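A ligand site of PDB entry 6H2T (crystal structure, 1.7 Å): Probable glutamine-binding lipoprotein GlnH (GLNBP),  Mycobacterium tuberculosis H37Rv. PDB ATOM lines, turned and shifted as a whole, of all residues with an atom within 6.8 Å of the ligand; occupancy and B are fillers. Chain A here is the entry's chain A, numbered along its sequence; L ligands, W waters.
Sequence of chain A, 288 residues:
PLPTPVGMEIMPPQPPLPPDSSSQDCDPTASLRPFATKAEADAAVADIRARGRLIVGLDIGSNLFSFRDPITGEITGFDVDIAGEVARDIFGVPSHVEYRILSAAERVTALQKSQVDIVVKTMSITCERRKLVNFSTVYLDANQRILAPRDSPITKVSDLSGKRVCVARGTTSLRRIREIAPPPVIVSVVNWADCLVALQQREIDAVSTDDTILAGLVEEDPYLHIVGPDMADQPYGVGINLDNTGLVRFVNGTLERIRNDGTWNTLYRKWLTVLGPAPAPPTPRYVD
The side-chain carboxylate of Asp 210 is in salt-bridge range of a nitrogen (N1) of the ligand, 2.7 Å away. The backbone carbonyl oxygen (O) of Thr 122 lies within hydrogen-bond range of a nitrogen (N1) of the ligand (2.7 Å). O3 of the ligand is in hydrogen-bond range of OG1 of Thr 122 (2.9 Å). The guanidinium group (NH1) of Arg 107 lies within salt-bridge range of an oxygen (O3) of the ligand, 2.8 Å away. An oxygen (O2) of the ligand is in hydrogen-bond range of the indole nitrogen (NE1) of Trp 192. NH1 of Arg 129 lies within salt-bridge range of O4 of the ligand, at 2.8 Å. N of Ser 124 sits at hydrogen-bond distance from O4 of the ligand, at 2.9 Å. OG of Ser 124 lies within hydrogen-bond range of N1 of the ligand (2.9 Å). The backbone NH (N) of Thr 172 is in hydrogen-bond range of an oxygen (O1) of the ligand (2.9 Å).
The side-chain hydroxyl (OH) of Tyr 236 is in hydrogen-bond range of the side-chain carboxylate (OD2) of Asp 210 (2.6 Å). The backbone carbonyl oxygen of Ala 104 is in hydrogen-bond range of the guanidinium group of Arg 107 (3.0 Å). The guanidinium group of Arg 129 sits at hydrogen-bond distance from the backbone carbonyl oxygen of Ser 124, at 2.9 Å. OG of Ser 124 is in hydrogen-bond range of OE1 of Gln 234 (2.7 Å). The side-chain hydroxyl (OG1) of Thr 172 sits at hydrogen-bond distance from the side-chain amide oxygen (OE1) of Gln 234 (2.7 Å). The backbone NH (N) of Leu 174 lies within hydrogen-bond range of the side-chain hydroxyl (OG1) of Thr 171, 3.3 Å away. The side-chain hydroxyl (OG) of Ser 173 sits at hydrogen-bond distance from the side-chain hydroxyl (OG1) of Thr 209 (2.7 Å). The backbone NH (N) of Gln 234 sits at hydrogen-bond distance from the backbone carbonyl oxygen (O) of Ala 142.
Merely in contact with the ligand: Ala 104, Lys 121, Met 123, Thr 171, Ser 173, Thr 209, Ile 213, Gln 234 and Tyr 236. 16 residues have an atom within 4 Å of the ligand: Ala 104, Arg 107, Lys 121, Thr 122, Met 123, Ser 124, Arg 129, Thr 171, Thr 172, Ser 173, Trp 192, Thr 209, Asp 210, Ile 213, Gln 234 and Tyr 236. The nearest printed residue that does not touch the ligand is Gly 170 (4.3 Å).
Water W1 lies within hydrogen-bond range of NZ of Lys 121 (2.7 Å), O2 of the ligand (2.7 Å) and NH1 of Arg 107 (3.0 Å).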
ATOM      1  N   SER A  62     -26.966  17.893 -24.675  1.00  0.00           N
ATOM      2  CA  SER A  62     -26.548  19.005 -23.808  1.00  0.00           C
ATOM      3  C   SER A  62     -27.520  19.160 -22.652  1.00  0.00           C
ATOM      4  O   SER A  62     -28.487  19.926 -22.728  1.00  0.00           O
ATOM      5  CB  SER A  62     -26.433  20.300 -24.603  1.00  0.00           C
ATOM      6  OG  SER A  62     -25.408  20.191 -25.579  1.00  0.00           O
ATOM      7  N   ALA A 104     -23.365  19.600 -33.274  1.00  0.00           N
ATOM      8  CA  ALA A 104     -22.681  20.888 -33.322  1.00  0.00           C
ATOM      9  C   ALA A 104     -22.042  21.123 -34.686  1.00  0.00           C
ATOM     10  O   ALA A 104     -22.043  22.241 -35.197  1.00  0.00           O
ATOM     11  CB  ALA A 104     -21.620  20.963 -32.213  1.00  0.00           C
ATOM     12  N   ARG A 107     -24.602  22.497 -37.554  1.00  0.00           N
ATOM     13  CA  ARG A 107     -25.450  23.668 -37.371  1.00  0.00           C
ATOM     14  C   ARG A 107     -25.399  24.594 -38.587  1.00  0.00           C
ATOM     15  O   ARG A 107     -26.446  25.034 -39.090  1.00  0.00           O
ATOM     16  CB  ARG A 107     -25.028  24.418 -36.111  1.00  0.00           C
ATOM     17  CG  ARG A 107     -25.366  23.685 -34.821  1.00  0.00           C
ATOM     18  CD  ARG A 107     -24.822  24.467 -33.627  1.00  0.00           C
ATOM     19  NE  ARG A 107     -23.355  24.374 -33.589  1.00  0.00           N
ATOM     20  CZ  ARG A 107     -22.623  24.803 -32.569  1.00  0.00           C
ATOM     21  NH1 ARG A 107     -23.217  25.404 -31.539  1.00  0.00           N
ATOM     22  NH2 ARG A 107     -21.299  24.659 -32.608  1.00  0.00           N
ATOM     23  N   LYS A 121     -28.972  25.976 -30.263  1.00  0.00           N
ATOM     24  CA  LYS A 121     -28.119  24.889 -29.784  1.00  0.00           C
ATOM     25  C   LYS A 121     -26.777  25.502 -29.386  1.00  0.00           C
ATOM     26  O   LYS A 121     -25.776  25.350 -30.090  1.00  0.00           O
ATOM     27  CB  LYS A 121     -27.937  23.807 -30.845  1.00  0.00           C
ATOM     28  CG  LYS A 121     -27.399  22.493 -30.283  1.00  0.00           C
ATOM     29  CD  LYS A 121     -26.654  21.688 -31.352  1.00  0.00           C
ATOM     30  CE  LYS A 121     -26.142  20.378 -30.772  1.00  0.00           C
ATOM     31  NZ  LYS A 121     -25.159  20.592 -29.670  1.00  0.00           N
ATOM     32  N   THR A 122     -26.806  26.180 -28.231  1.00  0.00           N
ATOM     33  CA  THR A 122     -25.680  26.886 -27.617  1.00  0.00           C
ATOM     34  C   THR A 122     -24.740  27.501 -28.641  1.00  0.00           C
ATOM     35  O   THR A 122     -23.522  27.341 -28.535  1.00  0.00           O
ATOM     36  CB  THR A 122     -24.902  25.945 -26.678  1.00  0.00           C
ATOM     37  OG1 THR A 122     -24.420  24.787 -27.380  1.00  0.00           O
ATOM     38  CG2 THR A 122     -25.792  25.485 -25.520  1.00  0.00           C
ATOM     39  N   MET A 123     -25.270  28.237 -29.618  1.00  0.00           N
ATOM     40  CA  MET A 123     -24.486  28.565 -30.804  1.00  0.00           C
ATOM     41  C   MET A 123     -23.773  29.894 -30.619  1.00  0.00           C
ATOM     42  O   MET A 123     -24.373  30.966 -30.740  1.00  0.00           O
ATOM     43  CB  MET A 123     -25.368  28.586 -32.044  1.00  0.00           C
ATOM     44  CG  MET A 123     -24.532  28.561 -33.307  1.00  0.00           C
ATOM     45  SD  MET A 123     -25.550  28.257 -34.749  1.00  0.00           S
ATOM     46  CE  MET A 123     -24.307  28.247 -36.037  1.00  0.00           C
ATOM     47  N   SER A 124     -22.462  29.826 -30.362  1.00  0.00           N
ATOM     48  CA  SER A 124     -21.665  31.041 -30.208  1.00  0.00           C
ATOM     49  C   SER A 124     -21.674  31.876 -31.489  1.00  0.00           C
ATOM     50  O   SER A 124     -21.468  31.345 -32.596  1.00  0.00           O
ATOM     51  CB  SER A 124     -20.238  30.685 -29.813  1.00  0.00           C
ATOM     52  OG  SER A 124     -20.260  30.151 -28.495  1.00  0.00           O
ATOM     53  N   ILE A 125     -21.890  33.174 -31.334  1.00  0.00           N
ATOM     54  CA  ILE A 125     -21.852  34.119 -32.437  1.00  0.00           C
ATOM     55  C   ILE A 125     -20.405  34.502 -32.697  1.00  0.00           C
ATOM     56  O   ILE A 125     -19.737  35.059 -31.821  1.00  0.00           O
ATOM     57  CB  ILE A 125     -22.681  35.374 -32.128  1.00  0.00           C
ATOM     58  CG1 ILE A 125     -24.128  34.991 -31.785  1.00  0.00           C
ATOM     59  CG2 ILE A 125     -22.604  36.368 -33.290  1.00  0.00           C
ATOM     60  CD1 ILE A 125     -24.878  36.074 -31.016  1.00  0.00           C
ATOM     61  N   THR A 126     -19.902  34.222 -33.902  1.00  0.00           N
ATOM     62  CA  THR A 126     -18.525  34.537 -34.246  1.00  0.00           C
ATOM     63  C   THR A 126     -18.479  35.197 -35.618  1.00  0.00           C
ATOM     64  O   THR A 126     -19.375  35.038 -36.447  1.00  0.00           O
ATOM     65  CB  THR A 126     -17.604  33.301 -34.278  1.00  0.00           C
ATOM     66  OG1 THR A 126     -17.938  32.482 -35.402  1.00  0.00           O
ATOM     67  CG2 THR A 126     -17.728  32.486 -32.975  1.00  0.00           C
ATOM     68  N   ARG A 129     -18.430  32.533 -38.370  1.00  0.00           N
ATOM     69  CA  ARG A 129     -19.764  31.997 -38.646  1.00  0.00           C
ATOM     70  C   ARG A 129     -20.660  33.013 -39.339  1.00  0.00           C
ATOM     71  O   ARG A 129     -21.494  32.621 -40.167  1.00  0.00           O
ATOM     72  CB  ARG A 129     -20.409  31.497 -37.355  1.00  0.00           C
ATOM     73  CG  ARG A 129     -19.740  30.230 -36.862  1.00  0.00           C
ATOM     74  CD  ARG A 129     -20.139  29.931 -35.442  1.00  0.00           C
ATOM     75  NE  ARG A 129     -19.471  28.717 -34.999  1.00  0.00           N
ATOM     76  CZ  ARG A 129     -19.745  28.091 -33.856  1.00  0.00           C
ATOM     77  NH1 ARG A 129     -20.671  28.578 -33.024  1.00  0.00           N
ATOM     78  NH2 ARG A 129     -19.069  26.994 -33.538  1.00  0.00           N
ATOM     79  N   ALA A 142     -21.930  32.822 -22.141  1.00  0.00           N
ATOM     80  CA  ALA A 142     -21.182  31.816 -21.383  1.00  0.00           C
ATOM     81  C   ALA A 142     -19.679  32.039 -21.553  1.00  0.00           C
ATOM     82  O   ALA A 142     -19.242  32.926 -22.288  1.00  0.00           O
ATOM     83  CB  ALA A 142     -21.589  30.408 -21.824  1.00  0.00           C
ATOM     84  N   GLN A 144     -15.852  29.635 -21.758  1.00  0.00           N
ATOM     85  CA  GLN A 144     -15.237  28.319 -21.792  1.00  0.00           C
ATOM     86  C   GLN A 144     -14.414  28.080 -20.527  1.00  0.00           C
ATOM     87  O   GLN A 144     -13.625  28.927 -20.126  1.00  0.00           O
ATOM     88  CB  GLN A 144     -14.327  28.203 -23.021  1.00  0.00           C
ATOM     89  CG  GLN A 144     -13.688  26.827 -23.090  1.00  0.00           C
ATOM     90  CD  GLN A 144     -13.131  26.548 -24.467  1.00  0.00           C
ATOM     91  OE1 GLN A 144     -13.380  27.302 -25.405  1.00  0.00           O
ATOM     92  NE2 GLN A 144     -12.363  25.481 -24.584  1.00  0.00           N
ATOM     93  N   ALA A 168     -16.562  18.411 -28.433  1.00  0.00           N
ATOM     94  CA  ALA A 168     -17.352  18.013 -29.603  1.00  0.00           C
ATOM     95  C   ALA A 168     -16.776  18.629 -30.883  1.00  0.00           C
ATOM     96  O   ALA A 168     -16.323  19.767 -30.891  1.00  0.00           O
ATOM     97  CB  ALA A 168     -18.813  18.443 -29.412  1.00  0.00           C
ATOM     98  N   ARG A 169     -16.822  17.857 -31.969  1.00  0.00           N
ATOM     99  CA  ARG A 169     -16.404  18.374 -33.264  1.00  0.00           C
ATOM    100  C   ARG A 169     -17.282  19.561 -33.674  1.00  0.00           C
ATOM    101  O   ARG A 169     -18.459  19.630 -33.316  1.00  0.00           O
ATOM    102  CB  ARG A 169     -16.467  17.279 -34.324  1.00  0.00           C
ATOM    103  CG  ARG A 169     -15.348  16.256 -34.123  1.00  0.00           C
ATOM    104  CD  ARG A 169     -15.287  15.235 -35.234  1.00  0.00           C
ATOM    105  NE  ARG A 169     -16.365  14.256 -35.117  1.00  0.00           N
ATOM    106  CZ  ARG A 169     -16.360  13.233 -34.261  1.00  0.00           C
ATOM    107  NH1 ARG A 169     -15.324  13.046 -33.444  1.00  0.00           N
ATOM    108  NH2 ARG A 169     -17.386  12.391 -34.232  1.00  0.00           N
ATOM    109  N   GLY A 170     -16.680  20.492 -34.416  1.00  0.00           N
ATOM    110  CA  GLY A 170     -17.436  21.616 -34.945  1.00  0.00           C
ATOM    111  C   GLY A 170     -17.725  22.727 -33.963  1.00  0.00           C
ATOM    112  O   GLY A 170     -18.698  23.466 -34.151  1.00  0.00           O
ATOM    113  N   THR A 171     -16.915  22.859 -32.914  1.00  0.00           N
ATOM    114  CA  THR A 171     -17.182  23.815 -31.850  1.00  0.00           C
ATOM    115  C   THR A 171     -16.059  24.835 -31.724  1.00  0.00           C
ATOM    116  O   THR A 171     -14.902  24.596 -32.115  1.00  0.00           O
ATOM    117  CB  THR A 171     -17.355  23.114 -30.485  1.00  0.00           C
ATOM    118  OG1 THR A 171     -16.164  22.369 -30.175  1.00  0.00           O
ATOM    119  CG2 THR A 171     -18.557  22.196 -30.514  1.00  0.00           C
ATOM    120  N   THR A 172     -16.421  25.995 -31.159  1.00  0.00           N
ATOM    121  CA  THR A 172     -15.387  26.955 -30.768  1.00  0.00           C
ATOM    122  C   THR A 172     -14.474  26.367 -29.708  1.00  0.00           C
ATOM    123  O   THR A 172     -13.308  26.772 -29.596  1.00  0.00           O
ATOM    124  CB  THR A 172     -16.016  28.246 -30.230  1.00  0.00           C
ATOM    125  OG1 THR A 172     -16.784  27.926 -29.057  1.00  0.00           O
ATOM    126  CG2 THR A 172     -16.929  28.883 -31.279  1.00  0.00           C
ATOM    127  N   SER A 173     -14.995  25.422 -28.922  1.00  0.00           N
ATOM    128  CA  SER A 173     -14.215  24.819 -27.850  1.00  0.00           C
ATOM    129  C   SER A 173     -12.970  24.162 -28.380  1.00  0.00           C
ATOM    130  O   SER A 173     -11.888  24.293 -27.805  1.00  0.00           O
ATOM    131  CB  SER A 173     -15.077  23.789 -27.106  1.00  0.00           C
ATOM    132  OG  SER A 173     -16.347  24.353 -26.776  1.00  0.00           O
ATOM    133  N   LEU A 174     -13.106  23.437 -29.498  1.00  0.00           N
ATOM    134  CA  LEU A 174     -11.961  22.806 -30.148  1.00  0.00           C
ATOM    135  C   LEU A 174     -10.944  23.849 -30.587  1.00  0.00           C
ATOM    136  O   LEU A 174      -9.733  23.706 -30.326  1.00  0.00           O
ATOM    137  CB  LEU A 174     -12.446  21.970 -31.337  1.00  0.00           C
ATOM    138  CG  LEU A 174     -11.380  21.436 -32.293  1.00  0.00           C
ATOM    139  CD1 LEU A 174     -10.368  20.611 -31.504  1.00  0.00           C
ATOM    140  CD2 LEU A 174     -12.046  20.605 -33.391  1.00  0.00           C
ATOM    141  N   TRP A 192     -21.858  16.626 -26.397  1.00  0.00           N
ATOM    142  CA  TRP A 192     -21.231  16.851 -25.100  1.00  0.00           C
ATOM    143  C   TRP A 192     -21.518  15.712 -24.132  1.00  0.00           C
ATOM    144  O   TRP A 192     -20.675  15.392 -23.288  1.00  0.00           O
ATOM    145  CB  TRP A 192     -21.653  18.216 -24.567  1.00  0.00           C
ATOM    146  CG  TRP A 192     -21.032  19.286 -25.430  1.00  0.00           C
ATOM    147  CD1 TRP A 192     -21.657  20.103 -26.328  1.00  0.00           C
ATOM    148  CD2 TRP A 192     -19.635  19.583 -25.524  1.00  0.00           C
ATOM    149  NE1 TRP A 192     -20.735  20.915 -26.956  1.00  0.00           N
ATOM    150  CE2 TRP A 192     -19.483  20.615 -26.477  1.00  0.00           C
ATOM    151  CE3 TRP A 192     -18.491  19.088 -24.887  1.00  0.00           C
ATOM    152  CZ2 TRP A 192     -18.238  21.157 -26.811  1.00  0.00           C
ATOM    153  CZ3 TRP A 192     -17.245  19.617 -25.222  1.00  0.00           C
ATOM    154  CH2 TRP A 192     -17.138  20.639 -26.181  1.00  0.00           C
ATOM    155  N   THR A 209     -15.315  23.248 -22.384  1.00  0.00           N
ATOM    156  CA  THR A 209     -16.307  23.935 -23.204  1.00  0.00           C
ATOM    157  C   THR A 209     -17.015  24.955 -22.334  1.00  0.00           C
ATOM    158  O   THR A 209     -16.601  25.223 -21.196  1.00  0.00           O
ATOM    159  CB  THR A 209     -17.287  22.941 -23.859  1.00  0.00           C
ATOM    160  OG1 THR A 209     -18.082  23.642 -24.836  1.00  0.00           O
ATOM    161  CG2 THR A 209     -18.219  22.283 -22.825  1.00  0.00           C
ATOM    162  N   ASP A 210     -18.086  25.531 -22.873  1.00  0.00           N
ATOM    163  CA  ASP A 210     -18.893  26.539 -22.185  1.00  0.00           C
ATOM    164  C   ASP A 210     -19.227  26.088 -20.767  1.00  0.00           C
ATOM    165  O   ASP A 210     -19.695  24.969 -20.563  1.00  0.00           O
ATOM    166  CB  ASP A 210     -20.199  26.751 -22.943  1.00  0.00           C
ATOM    167  CG  ASP A 210     -20.010  27.070 -24.405  1.00  0.00           C
ATOM    168  OD1 ASP A 210     -18.859  27.206 -24.877  1.00  0.00           O
ATOM    169  OD2 ASP A 210     -21.049  27.163 -25.104  1.00  0.00           O
ATOM    170  N   ILE A 213     -22.631  24.482 -20.390  1.00  0.00           N
ATOM    171  CA  ILE A 213     -22.710  23.055 -20.729  1.00  0.00           C
ATOM    172  C   ILE A 213     -22.022  22.207 -19.667  1.00  0.00           C
ATOM    173  O   ILE A 213     -22.529  21.150 -19.270  1.00  0.00           O
ATOM    174  CB  ILE A 213     -22.102  22.830 -22.129  1.00  0.00           C
ATOM    175  CG1 ILE A 213     -22.970  23.513 -23.193  1.00  0.00           C
ATOM    176  CG2 ILE A 213     -21.894  21.320 -22.407  1.00  0.00           C
ATOM    177  CD1 ILE A 213     -22.289  23.615 -24.558  1.00  0.00           C
ATOM    178  N   GLN A 234     -18.398  33.193 -24.961  1.00  0.00           N
ATOM    179  CA  GLN A 234     -19.304  32.432 -25.828  1.00  0.00           C
ATOM    180  C   GLN A 234     -20.685  33.078 -25.807  1.00  0.00           C
ATOM    181  O   GLN A 234     -21.561  32.697 -25.021  1.00  0.00           O
ATOM    182  CB  GLN A 234     -19.408  30.980 -25.379  1.00  0.00           C
ATOM    183  CG  GLN A 234     -18.077  30.309 -25.110  1.00  0.00           C
ATOM    184  CD  GLN A 234     -17.264  30.048 -26.371  1.00  0.00           C
ATOM    185  OE1 GLN A 234     -17.794  29.828 -27.462  1.00  0.00           O
ATOM    186  NE2 GLN A 234     -15.952  30.052 -26.208  1.00  0.00           N
ATOM    187  N   PRO A 235     -20.926  34.055 -26.675  1.00  0.00           N
ATOM    188  CA  PRO A 235     -22.241  34.694 -26.709  1.00  0.00           C
ATOM    189  C   PRO A 235     -23.205  33.947 -27.613  1.00  0.00           C
ATOM    190  O   PRO A 235     -23.001  33.879 -28.830  1.00  0.00           O
ATOM    191  CB  PRO A 235     -21.939  36.105 -27.235  1.00  0.00           C
ATOM    192  CG  PRO A 235     -20.719  35.902 -28.139  1.00  0.00           C
ATOM    193  CD  PRO A 235     -19.969  34.686 -27.621  1.00  0.00           C
ATOM    194  N   TYR A 236     -24.258  33.374 -27.029  1.00  0.00           N
ATOM    195  CA  TYR A 236     -25.173  32.511 -27.769  1.00  0.00           C
ATOM    196  C   TYR A 236     -26.130  33.343 -28.609  1.00  0.00           C
ATOM    197  O   TYR A 236     -26.755  34.281 -28.108  1.00  0.00           O
ATOM    198  CB  TYR A 236     -26.021  31.652 -26.839  1.00  0.00           C
ATOM    199  CG  TYR A 236     -25.286  30.580 -26.072  1.00  0.00           C
ATOM    200  CD1 TYR A 236     -23.926  30.357 -26.258  1.00  0.00           C
ATOM    201  CD2 TYR A 236     -25.966  29.795 -25.163  1.00  0.00           C
ATOM    202  CE1 TYR A 236     -23.255  29.363 -25.531  1.00  0.00           C
ATOM    203  CE2 TYR A 236     -25.313  28.808 -24.452  1.00  0.00           C
ATOM    204  CZ  TYR A 236     -23.973  28.592 -24.637  1.00  0.00           C
ATOM    205  OH  TYR A 236     -23.353  27.604 -23.929  1.00  0.00           O
HETATM  206  N1  LIG L   1     -20.889  27.395 -27.779  1.00  0.00           N
HETATM  207  C1  LIG L   1     -19.697  26.853 -28.456  1.00  0.00           C
HETATM  208  C2  LIG L   1     -19.948  26.727 -29.958  1.00  0.00           C
HETATM  209  O1  LIG L   1     -19.300  25.956 -30.679  1.00  0.00           O
HETATM  210  C3  LIG L   1     -19.292  25.487 -27.862  1.00  0.00           C
HETATM  211  C4  LIG L   1     -20.442  24.610 -27.371  1.00  0.00           C
HETATM  212  C5  LIG L   1     -21.355  24.131 -28.484  1.00  0.00           C
HETATM  213  O2  LIG L   1     -21.419  22.897 -28.742  1.00  0.00           O
HETATM  214  O3  LIG L   1     -22.033  24.980 -29.088  1.00  0.00           O
HETATM  215  O4  LIG L   1     -20.836  27.424 -30.469  1.00  0.00           O
HETATM  216  O   HOH W   1     -23.694  22.778 -30.274  1.00  0.00           O
